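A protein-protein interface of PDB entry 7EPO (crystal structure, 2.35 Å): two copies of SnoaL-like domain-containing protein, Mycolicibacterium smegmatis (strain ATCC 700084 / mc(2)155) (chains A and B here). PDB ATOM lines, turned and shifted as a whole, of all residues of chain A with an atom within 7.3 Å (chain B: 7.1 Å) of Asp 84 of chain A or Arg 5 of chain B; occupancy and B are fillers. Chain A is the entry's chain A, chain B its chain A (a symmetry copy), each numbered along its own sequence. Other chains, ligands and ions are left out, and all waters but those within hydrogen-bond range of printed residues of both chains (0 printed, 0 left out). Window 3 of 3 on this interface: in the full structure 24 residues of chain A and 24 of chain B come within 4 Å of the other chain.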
ATOM      1  N   THR A   4      13.789 -24.001 -16.688  1.00  0.00           N
ATOM      2  CA  THR A   4      12.717 -23.014 -16.717  1.00  0.00           C
ATOM      3  C   THR A   4      12.861 -22.030 -15.563  1.00  0.00           C
ATOM      4  O   THR A   4      12.768 -20.810 -15.757  1.00  0.00           O
ATOM      5  CB  THR A   4      11.361 -23.717 -16.653  1.00  0.00           C
ATOM      6  OG1 THR A   4      11.272 -24.674 -17.712  1.00  0.00           O
ATOM      7  CG2 THR A   4      10.241 -22.709 -16.822  1.00  0.00           C
ATOM      8  N   ARG A   5      13.132 -22.551 -14.355  1.00  0.00           N
ATOM      9  CA  ARG A   5      13.161 -21.713 -13.160  1.00  0.00           C
ATOM     10  C   ARG A   5      14.362 -20.781 -13.167  1.00  0.00           C
ATOM     11  O   ARG A   5      14.245 -19.604 -12.801  1.00  0.00           O
ATOM     12  CB  ARG A   5      13.172 -22.577 -11.903  1.00  0.00           C
ATOM     13  CG  ARG A   5      13.072 -21.776 -10.631  1.00  0.00           C
ATOM     14  CD  ARG A   5      13.085 -22.669  -9.406  1.00  0.00           C
ATOM     15  NE  ARG A   5      11.785 -23.273  -9.115  1.00  0.00           N
ATOM     16  CZ  ARG A   5      10.779 -22.640  -8.518  1.00  0.00           C
ATOM     17  NH1 ARG A   5      10.913 -21.370  -8.165  1.00  0.00           N
ATOM     18  NH2 ARG A   5       9.636 -23.275  -8.277  1.00  0.00           N
ATOM     19  N   LEU A  82       5.972 -20.265  -9.067  1.00  0.00           N
ATOM     20  CA  LEU A  82       5.560 -21.638  -9.301  1.00  0.00           C
ATOM     21  C   LEU A  82       6.054 -22.041 -10.681  1.00  0.00           C
ATOM     22  O   LEU A  82       5.912 -21.268 -11.638  1.00  0.00           O
ATOM     23  CB  LEU A  82       4.039 -21.765  -9.215  1.00  0.00           C
ATOM     24  CG  LEU A  82       3.323 -21.159  -8.002  1.00  0.00           C
ATOM     25  CD1 LEU A  82       1.935 -21.762  -7.867  1.00  0.00           C
ATOM     26  CD2 LEU A  82       4.114 -21.353  -6.688  1.00  0.00           C
ATOM     27  N   VAL A  83       6.673 -23.224 -10.771  1.00  0.00           N
ATOM     28  CA  VAL A  83       7.205 -23.749 -12.027  1.00  0.00           C
ATOM     29  C   VAL A  83       6.626 -25.141 -12.253  1.00  0.00           C
ATOM     30  O   VAL A  83       6.633 -25.974 -11.341  1.00  0.00           O
ATOM     31  CB  VAL A  83       8.746 -23.789 -12.020  1.00  0.00           C
ATOM     32  CG1 VAL A  83       9.299 -24.090 -13.416  1.00  0.00           C
ATOM     33  CG2 VAL A  83       9.300 -22.472 -11.514  1.00  0.00           C
ATOM     34  N   ASP A  84       6.103 -25.387 -13.472  1.00  0.00           N
ATOM     35  CA  ASP A  84       5.517 -26.682 -13.868  1.00  0.00           C
ATOM     36  C   ASP A  84       5.893 -26.908 -15.338  1.00  0.00           C
ATOM     37  O   ASP A  84       5.112 -26.662 -16.263  1.00  0.00           O
ATOM     38  CB  ASP A  84       3.999 -26.716 -13.644  1.00  0.00           C
ATOM     39  CG  ASP A  84       3.374 -28.066 -13.971  1.00  0.00           C
ATOM     40  OD1 ASP A  84       4.100 -29.087 -14.057  1.00  0.00           O
ATOM     41  OD2 ASP A  84       2.132 -28.103 -14.127  1.00  0.00           O
ATOM     42  N   GLY A  85       7.111 -27.365 -15.547  1.00  0.00           N
ATOM     43  CA  GLY A  85       7.591 -27.706 -16.885  1.00  0.00           C
ATOM     44  C   GLY A  85       8.173 -26.491 -17.597  1.00  0.00           C
ATOM     45  O   GLY A  85       9.109 -25.864 -17.097  1.00  0.00           O
ATOM     46  N   ALA A  86       7.634 -26.182 -18.769  1.00  0.00           N
ATOM     47  CA  ALA A  86       8.073 -25.003 -19.488  1.00  0.00           C
ATOM     48  C   ALA A  86       7.347 -23.748 -19.026  1.00  0.00           C
ATOM     49  O   ALA A  86       7.683 -22.652 -19.485  1.00  0.00           O
ATOM     50  CB  ALA A  86       7.881 -25.203 -20.992  1.00  0.00           C
ATOM     51  N   ASP A  87       6.382 -23.884 -18.119  1.00  0.00           N
ATOM     52  CA  ASP A  87       5.518 -22.783 -17.724  1.00  0.00           C
ATOM     53  C   ASP A  87       5.782 -22.394 -16.278  1.00  0.00           C
ATOM     54  O   ASP A  87       6.085 -23.247 -15.441  1.00  0.00           O
ATOM     55  CB  ASP A  87       4.046 -23.150 -17.929  1.00  0.00           C
ATOM     56  CG  ASP A  87       3.645 -23.126 -19.388  1.00  0.00           C
ATOM     57  OD1 ASP A  87       3.760 -22.050 -20.010  1.00  0.00           O
ATOM     58  OD2 ASP A  87       3.213 -24.169 -19.914  1.00  0.00           O
ATOM     59  N   ALA A  88       5.689 -21.095 -16.003  1.00  0.00           N
ATOM     60  CA  ALA A  88       5.890 -20.562 -14.667  1.00  0.00           C
ATOM     61  C   ALA A  88       4.889 -19.446 -14.396  1.00  0.00           C
ATOM     62  O   ALA A  88       4.397 -18.788 -15.319  1.00  0.00           O
ATOM     63  CB  ALA A  88       7.312 -20.018 -14.469  1.00  0.00           C
ATOM     64  N   VAL A  89       4.583 -19.241 -13.115  1.00  0.00           N
ATOM     65  CA  VAL A  89       3.741 -18.135 -12.688  1.00  0.00           C
ATOM     66  C   VAL A  89       4.459 -17.374 -11.581  1.00  0.00           C
ATOM     67  O   VAL A  89       4.716 -17.926 -10.509  1.00  0.00           O
ATOM     68  CB  VAL A  89       2.360 -18.598 -12.206  1.00  0.00           C
ATOM     69  CG1 VAL A  89       1.606 -17.396 -11.643  1.00  0.00           C
ATOM     70  CG2 VAL A  89       1.596 -19.240 -13.350  1.00  0.00           C
ATOM     71  N   LEU A 113       4.480 -17.240 -17.452  1.00  0.00           N
ATOM     72  CA  LEU A 113       5.561 -17.310 -18.421  1.00  0.00           C
ATOM     73  C   LEU A 113       5.707 -18.719 -18.973  1.00  0.00           C
ATOM     74  O   LEU A 113       5.468 -19.712 -18.271  1.00  0.00           O
ATOM     75  CB  LEU A 113       6.880 -16.873 -17.813  1.00  0.00           C
ATOM     76  CG  LEU A 113       6.953 -15.432 -17.312  1.00  0.00           C
ATOM     77  CD1 LEU A 113       8.181 -15.222 -16.437  1.00  0.00           C
ATOM     78  CD2 LEU A 113       6.974 -14.484 -18.491  1.00  0.00           C
ATOM     79  N   VAL B   2      -4.452 -37.263  -1.030  1.00  0.00           N
ATOM     80  CA  VAL B   2      -4.065 -37.485  -2.414  1.00  0.00           C
ATOM     81  C   VAL B   2      -3.585 -36.172  -3.044  1.00  0.00           C
ATOM     82  O   VAL B   2      -3.530 -35.149  -2.371  1.00  0.00           O
ATOM     83  CB  VAL B   2      -5.216 -38.103  -3.195  1.00  0.00           C
ATOM     84  CG1 VAL B   2      -5.514 -39.497  -2.642  1.00  0.00           C
ATOM     85  CG2 VAL B   2      -6.444 -37.193  -3.114  1.00  0.00           C
ATOM     86  N   SER B   3      -3.271 -36.200  -4.338  1.00  0.00           N
ATOM     87  CA  SER B   3      -2.367 -35.225  -4.948  1.00  0.00           C
ATOM     88  C   SER B   3      -2.908 -33.795  -4.877  1.00  0.00           C
ATOM     89  O   SER B   3      -4.077 -33.544  -4.576  1.00  0.00           O
ATOM     90  CB  SER B   3      -2.095 -35.564  -6.418  1.00  0.00           C
ATOM     91  OG  SER B   3      -2.881 -34.796  -7.299  1.00  0.00           O
ATOM     92  N   THR B   4      -2.009 -32.843  -5.128  1.00  0.00           N
ATOM     93  CA  THR B   4      -2.426 -31.461  -5.325  1.00  0.00           C
ATOM     94  C   THR B   4      -3.273 -31.330  -6.584  1.00  0.00           C
ATOM     95  O   THR B   4      -4.342 -30.703  -6.566  1.00  0.00           O
ATOM     96  CB  THR B   4      -1.200 -30.553  -5.408  1.00  0.00           C
ATOM     97  OG1 THR B   4      -0.395 -30.735  -4.241  1.00  0.00           O
ATOM     98  CG2 THR B   4      -1.629 -29.100  -5.473  1.00  0.00           C
ATOM     99  N   ARG B   5      -2.821 -31.956  -7.684  1.00  0.00           N
ATOM    100  CA  ARG B   5      -3.484 -31.789  -8.974  1.00  0.00           C
ATOM    101  C   ARG B   5      -4.843 -32.470  -8.991  1.00  0.00           C
ATOM    102  O   ARG B   5      -5.816 -31.916  -9.521  1.00  0.00           O
ATOM    103  CB  ARG B   5      -2.607 -32.336 -10.097  1.00  0.00           C
ATOM    104  CG  ARG B   5      -3.173 -32.079 -11.469  1.00  0.00           C
ATOM    105  CD  ARG B   5      -2.274 -32.633 -12.557  1.00  0.00           C
ATOM    106  NE  ARG B   5      -1.141 -31.764 -12.874  1.00  0.00           N
ATOM    107  CZ  ARG B   5      -1.218 -30.676 -13.634  1.00  0.00           C
ATOM    108  NH1 ARG B   5      -2.384 -30.306 -14.142  1.00  0.00           N
ATOM    109  NH2 ARG B   5      -0.130 -29.953 -13.883  1.00  0.00           N
ATOM    110  N   GLU B   6      -4.927 -33.667  -8.413  1.00  0.00           N
ATOM    111  CA  GLU B   6      -6.211 -34.340  -8.262  1.00  0.00           C
ATOM    112  C   GLU B   6      -7.189 -33.466  -7.484  1.00  0.00           C
ATOM    113  O   GLU B   6      -8.338 -33.271  -7.905  1.00  0.00           O
ATOM    114  CB  GLU B   6      -6.006 -35.692  -7.567  1.00  0.00           C
ATOM    115  CG  GLU B   6      -5.144 -36.707  -8.342  1.00  0.00           C
ATOM    116  CD  GLU B   6      -4.589 -37.816  -7.439  1.00  0.00           C
ATOM    117  OE1 GLU B   6      -4.086 -38.844  -7.954  1.00  0.00           O
ATOM    118  OE2 GLU B   6      -4.646 -37.649  -6.206  1.00  0.00           O
ATOM    119  N   THR B   7      -6.746 -32.918  -6.348  1.00  0.00           N
ATOM    120  CA  THR B   7      -7.622 -32.043  -5.572  1.00  0.00           C
ATOM    121  C   THR B   7      -8.173 -30.912  -6.437  1.00  0.00           C
ATOM    122  O   THR B   7      -9.375 -30.617  -6.398  1.00  0.00           O
ATOM    123  CB  THR B   7      -6.882 -31.478  -4.356  1.00  0.00           C
ATOM    124  OG1 THR B   7      -6.306 -32.544  -3.586  1.00  0.00           O
ATOM    125  CG2 THR B   7      -7.834 -30.633  -3.478  1.00  0.00           C
ATOM    126  N   VAL B   8      -7.318 -30.299  -7.257  1.00  0.00           N
ATOM    127  CA  VAL B   8      -7.740 -29.130  -8.018  1.00  0.00           C
ATOM    128  C   VAL B   8      -8.754 -29.521  -9.081  1.00  0.00           C
ATOM    129  O   VAL B   8      -9.788 -28.861  -9.236  1.00  0.00           O
ATOM    130  CB  VAL B   8      -6.528 -28.422  -8.637  1.00  0.00           C
ATOM    131  CG1 VAL B   8      -6.991 -27.337  -9.567  1.00  0.00           C
ATOM    132  CG2 VAL B   8      -5.639 -27.859  -7.548  1.00  0.00           C
ATOM    133  N   ASN B   9      -8.466 -30.589  -9.837  1.00  0.00           N
ATOM    134  CA  ASN B   9      -9.390 -31.027 -10.882  1.00  0.00           C
ATOM    135  C   ASN B   9     -10.759 -31.344 -10.298  1.00  0.00           C
ATOM    136  O   ASN B   9     -11.793 -31.059 -10.915  1.00  0.00           O
ATOM    137  CB  ASN B   9      -8.835 -32.254 -11.624  1.00  0.00           C
ATOM    138  CG  ASN B   9      -7.585 -31.945 -12.444  1.00  0.00           C
ATOM    139  OD1 ASN B   9      -7.477 -30.901 -13.084  1.00  0.00           O
ATOM    140  ND2 ASN B   9      -6.641 -32.875 -12.437  1.00  0.00           N
ATOM    141  N   GLU B  10     -10.780 -31.946  -9.108  1.00  0.00           N
ATOM    142  CA  GLU B  10     -12.034 -32.163  -8.399  1.00  0.00           C
ATOM    143  C   GLU B  10     -12.712 -30.842  -8.044  1.00  0.00           C
ATOM    144  O   GLU B  10     -13.945 -30.763  -8.032  1.00  0.00           O
ATOM    145  CB  GLU B  10     -11.771 -33.000  -7.150  1.00  0.00           C
ATOM    146  CG  GLU B  10     -12.971 -33.223  -6.271  1.00  0.00           C
ATOM    147  CD  GLU B  10     -14.030 -34.046  -6.954  1.00  0.00           C
ATOM    148  OE1 GLU B  10     -13.701 -34.735  -7.945  1.00  0.00           O
ATOM    149  OE2 GLU B  10     -15.190 -34.010  -6.501  1.00  0.00           O
ATOM    150  N   LEU B  11     -11.929 -29.794  -7.756  1.00  0.00           N
ATOM    151  CA  LEU B  11     -12.523 -28.490  -7.473  1.00  0.00           C
ATOM    152  C   LEU B  11     -13.164 -27.904  -8.728  1.00  0.00           C
ATOM    153  O   LEU B  11     -14.311 -27.449  -8.693  1.00  0.00           O
ATOM    154  CB  LEU B  11     -11.466 -27.544  -6.886  1.00  0.00           C
ATOM    155  CG  LEU B  11     -11.939 -26.094  -6.674  1.00  0.00           C
ATOM    156  CD1 LEU B  11     -12.969 -25.995  -5.568  1.00  0.00           C
ATOM    157  CD2 LEU B  11     -10.768 -25.184  -6.352  1.00  0.00           C
ATOM    158  N   SER B  80      -5.283 -24.048 -18.739  1.00  0.00           N
ATOM    159  CA  SER B  80      -4.253 -24.928 -18.197  1.00  0.00           C
ATOM    160  C   SER B  80      -4.301 -24.904 -16.674  1.00  0.00           C
ATOM    161  O   SER B  80      -4.926 -24.040 -16.052  1.00  0.00           O
ATOM    162  CB  SER B  80      -2.854 -24.534 -18.687  1.00  0.00           C
ATOM    163  OG  SER B  80      -2.219 -23.677 -17.753  1.00  0.00           O
ATOM    164  N   VAL B  81      -3.617 -25.875 -16.078  1.00  0.00           N
ATOM    165  CA  VAL B  81      -3.478 -25.957 -14.634  1.00  0.00           C
ATOM    166  C   VAL B  81      -2.020 -26.273 -14.339  1.00  0.00           C
ATOM    167  O   VAL B  81      -1.553 -27.390 -14.602  1.00  0.00           O
ATOM    168  CB  VAL B  81      -4.405 -27.005 -14.011  1.00  0.00           C
ATOM    169  CG1 VAL B  81      -4.056 -27.201 -12.540  1.00  0.00           C
ATOM    170  CG2 VAL B  81      -5.846 -26.559 -14.168  1.00  0.00           C
ATOM    171  N   LEU B  82      -1.295 -25.290 -13.823  1.00  0.00           N
ATOM    172  CA  LEU B  82       0.095 -25.471 -13.441  1.00  0.00           C
ATOM    173  C   LEU B  82       0.123 -25.897 -11.982  1.00  0.00           C
ATOM    174  O   LEU B  82      -0.589 -25.313 -11.154  1.00  0.00           O
ATOM    175  CB  LEU B  82       0.880 -24.174 -13.638  1.00  0.00           C
ATOM    176  CG  LEU B  82       0.752 -23.440 -14.979  1.00  0.00           C
ATOM    177  CD1 LEU B  82       1.909 -22.470 -15.149  1.00  0.00           C
ATOM    178  CD2 LEU B  82       0.693 -24.409 -16.182  1.00  0.00           C
ATOM    179  N   VAL B  83       0.905 -26.940 -11.680  1.00  0.00           N
ATOM    180  CA  VAL B  83       1.036 -27.469 -10.324  1.00  0.00           C
ATOM    181  C   VAL B  83       2.516 -27.510  -9.962  1.00  0.00           C
ATOM    182  O   VAL B  83       3.337 -27.992 -10.749  1.00  0.00           O
ATOM    183  CB  VAL B  83       0.400 -28.868 -10.195  1.00  0.00           C
ATOM    184  CG1 VAL B  83       0.309 -29.302  -8.729  1.00  0.00           C
ATOM    185  CG2 VAL B  83      -0.978 -28.875 -10.825  1.00  0.00           C
ATOM    186  N   ASP B  84       2.861 -26.980  -8.770  1.00  0.00           N
ATOM    187  CA  ASP B  84       4.243 -26.950  -8.254  1.00  0.00           C
ATOM    188  C   ASP B  84       4.156 -27.184  -6.740  1.00  0.00           C
ATOM    189  O   ASP B  84       4.197 -26.255  -5.927  1.00  0.00           O
ATOM    190  CB  ASP B  84       4.954 -25.635  -8.599  1.00  0.00           C
ATOM    191  CG  ASP B  84       6.409 -25.602  -8.147  1.00  0.00           C
ATOM    192  OD1 ASP B  84       6.999 -26.674  -7.862  1.00  0.00           O
ATOM    193  OD2 ASP B  84       6.970 -24.485  -8.094  1.00  0.00           O
ATOM    194  N   GLY B  85       4.016 -28.440  -6.368  1.00  0.00           N
ATOM    195  CA  GLY B  85       3.998 -28.833  -4.960  1.00  0.00           C
ATOM    196  C   GLY B  85       2.595 -28.744  -4.372  1.00  0.00           C
ATOM    197  O   GLY B  85       1.668 -29.384  -4.871  1.00  0.00           O
ATOM    198  N   ALA B  88      -1.018 -24.449  -6.888  1.00  0.00           N
ATOM    199  CA  ALA B  88      -1.470 -24.585  -8.262  1.00  0.00           C
ATOM    200  C   ALA B  88      -2.010 -23.252  -8.766  1.00  0.00           C
ATOM    201  O   ALA B  88      -2.464 -22.408  -7.985  1.00  0.00           O
ATOM    202  CB  ALA B  88      -2.560 -25.654  -8.409  1.00  0.00           C
ATOM    203  N   VAL B 115      -3.031 -26.400  -1.497  1.00  0.00           N
ATOM    204  CA  VAL B 115      -3.705 -27.577  -0.973  1.00  0.00           C
ATOM    205  C   VAL B 115      -2.851 -28.163   0.142  1.00  0.00           C
ATOM    206  O   VAL B 115      -1.635 -28.305  -0.013  1.00  0.00           O
ATOM    207  CB  VAL B 115      -3.975 -28.619  -2.076  1.00  0.00           C
ATOM    208  CG1 VAL B 115      -4.513 -29.907  -1.466  1.00  0.00           C
ATOM    209  CG2 VAL B 115      -4.961 -28.053  -3.100  1.00  0.00           C
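Arg 5 of chain A touches Asp 84 of chain B, and with the chains exchanged Asp 84 of chain A touches Arg 5 of chain B.
Leu 82 of chain A touches Asp 84 of chain B, and with the chains exchanged Asp 84 of chain A touches Leu 82 of chain B.
Val 83 of chain A touches its own counterpart, Val 83 of chain B.
Val 83 of chain A touches Asp 84 of chain B, and with the chains exchanged Asp 84 of chain A touches Val 83 of chain B.
Positions printed for both chains: 4, 5, 82, 83, 84, 85 and 88.
Of the 10 pairs that touch across the chains among the printed residues, 7 have their exchanged pair printed and touching as well.
Among the printed residues, merely in contact across the chains: Asp 84 of chain A with Leu 82 of chain B (3.4 Å), Leu 82 of chain A with Asp 84 of chain B (3.4 Å), Asp 87 of chain A with Leu 82 of chain B (3.6 Å), Val 89 of chain A with Leu 82 of chain B (3.7 Å), Asp 84 of chain A with Val 81 of chain B (3.8 Å) and Val 83 of chain A with Val 83 of chain B (3.9 Å).
Among the printed residues, 10 pairs touch across the chains.
Among the printed residues, Asp or Glu carboxylates within 4 Å of a Lys or Arg side-chain nitrogen of the other chain: Arg 5 of chain A with Asp 84 of chain B (2.9 Å) and Asp 84 of chain A with Arg 5 of chain B (2.9 Å).
Asp 84 of chain A touches just these residues of chain B: Arg 5 (2.9 Å), Val 81 (3.8 Å), Leu 82 (3.4 Å) and Val 83 (3.0 Å).
Of chain A, only Asp 84 (2.9 Å) comes within 4 Å of Arg 5 of chain B.
Of the printed residues of chain B, Val 83 of chain A touches Val 83 (3.9 Å) and Asp 84 (3.0 Å).
Printed residues of chain B within 4 Å of Leu 82 of chain A: Asp 84.
The nearest residue of chain B that does not touch Asp 84 of chain A is Asp 84 of chain B (5.0 Å).
The backbone carbonyl oxygen of Leu 82 of chain A lies within hydrogen-bond range of the backbone NH of Val 89 of chain A (2.8 Å).
The backbone NH of Arg 5 of chain B is in hydrogen-bond range of the side-chain hydroxyl of Ser 3 of chain B, 2.9 Å away.
The backbone carbonyl oxygen of Arg 5 of chain B lies within hydrogen-bond range of the side-chain amide nitrogen of Asn 9 of chain B, 3.2 Å away.
The backbone carbonyl oxygen (O) of Val 81 of chain B is in hydrogen-bond range of the guanidinium group (NH2) of Arg 5 of chain B, 3.0 Å away.
NH2 of Arg 5 of chain A is in salt-bridge range of OD2 of Asp 84 of chain B (2.9 Å).
OD2 of Asp 84 of chain B sits at hydrogen-bond distance from N of Val 83 of chain A, at 3.0 Å.
NH2 of Arg 5 of chain B lies within salt-bridge range of OD2 of Asp 84 of chain A (2.9 Å).
The side-chain carboxylate of Asp 84 of chain A lies within hydrogen-bond range of the backbone NH of Val 83 of chain B.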
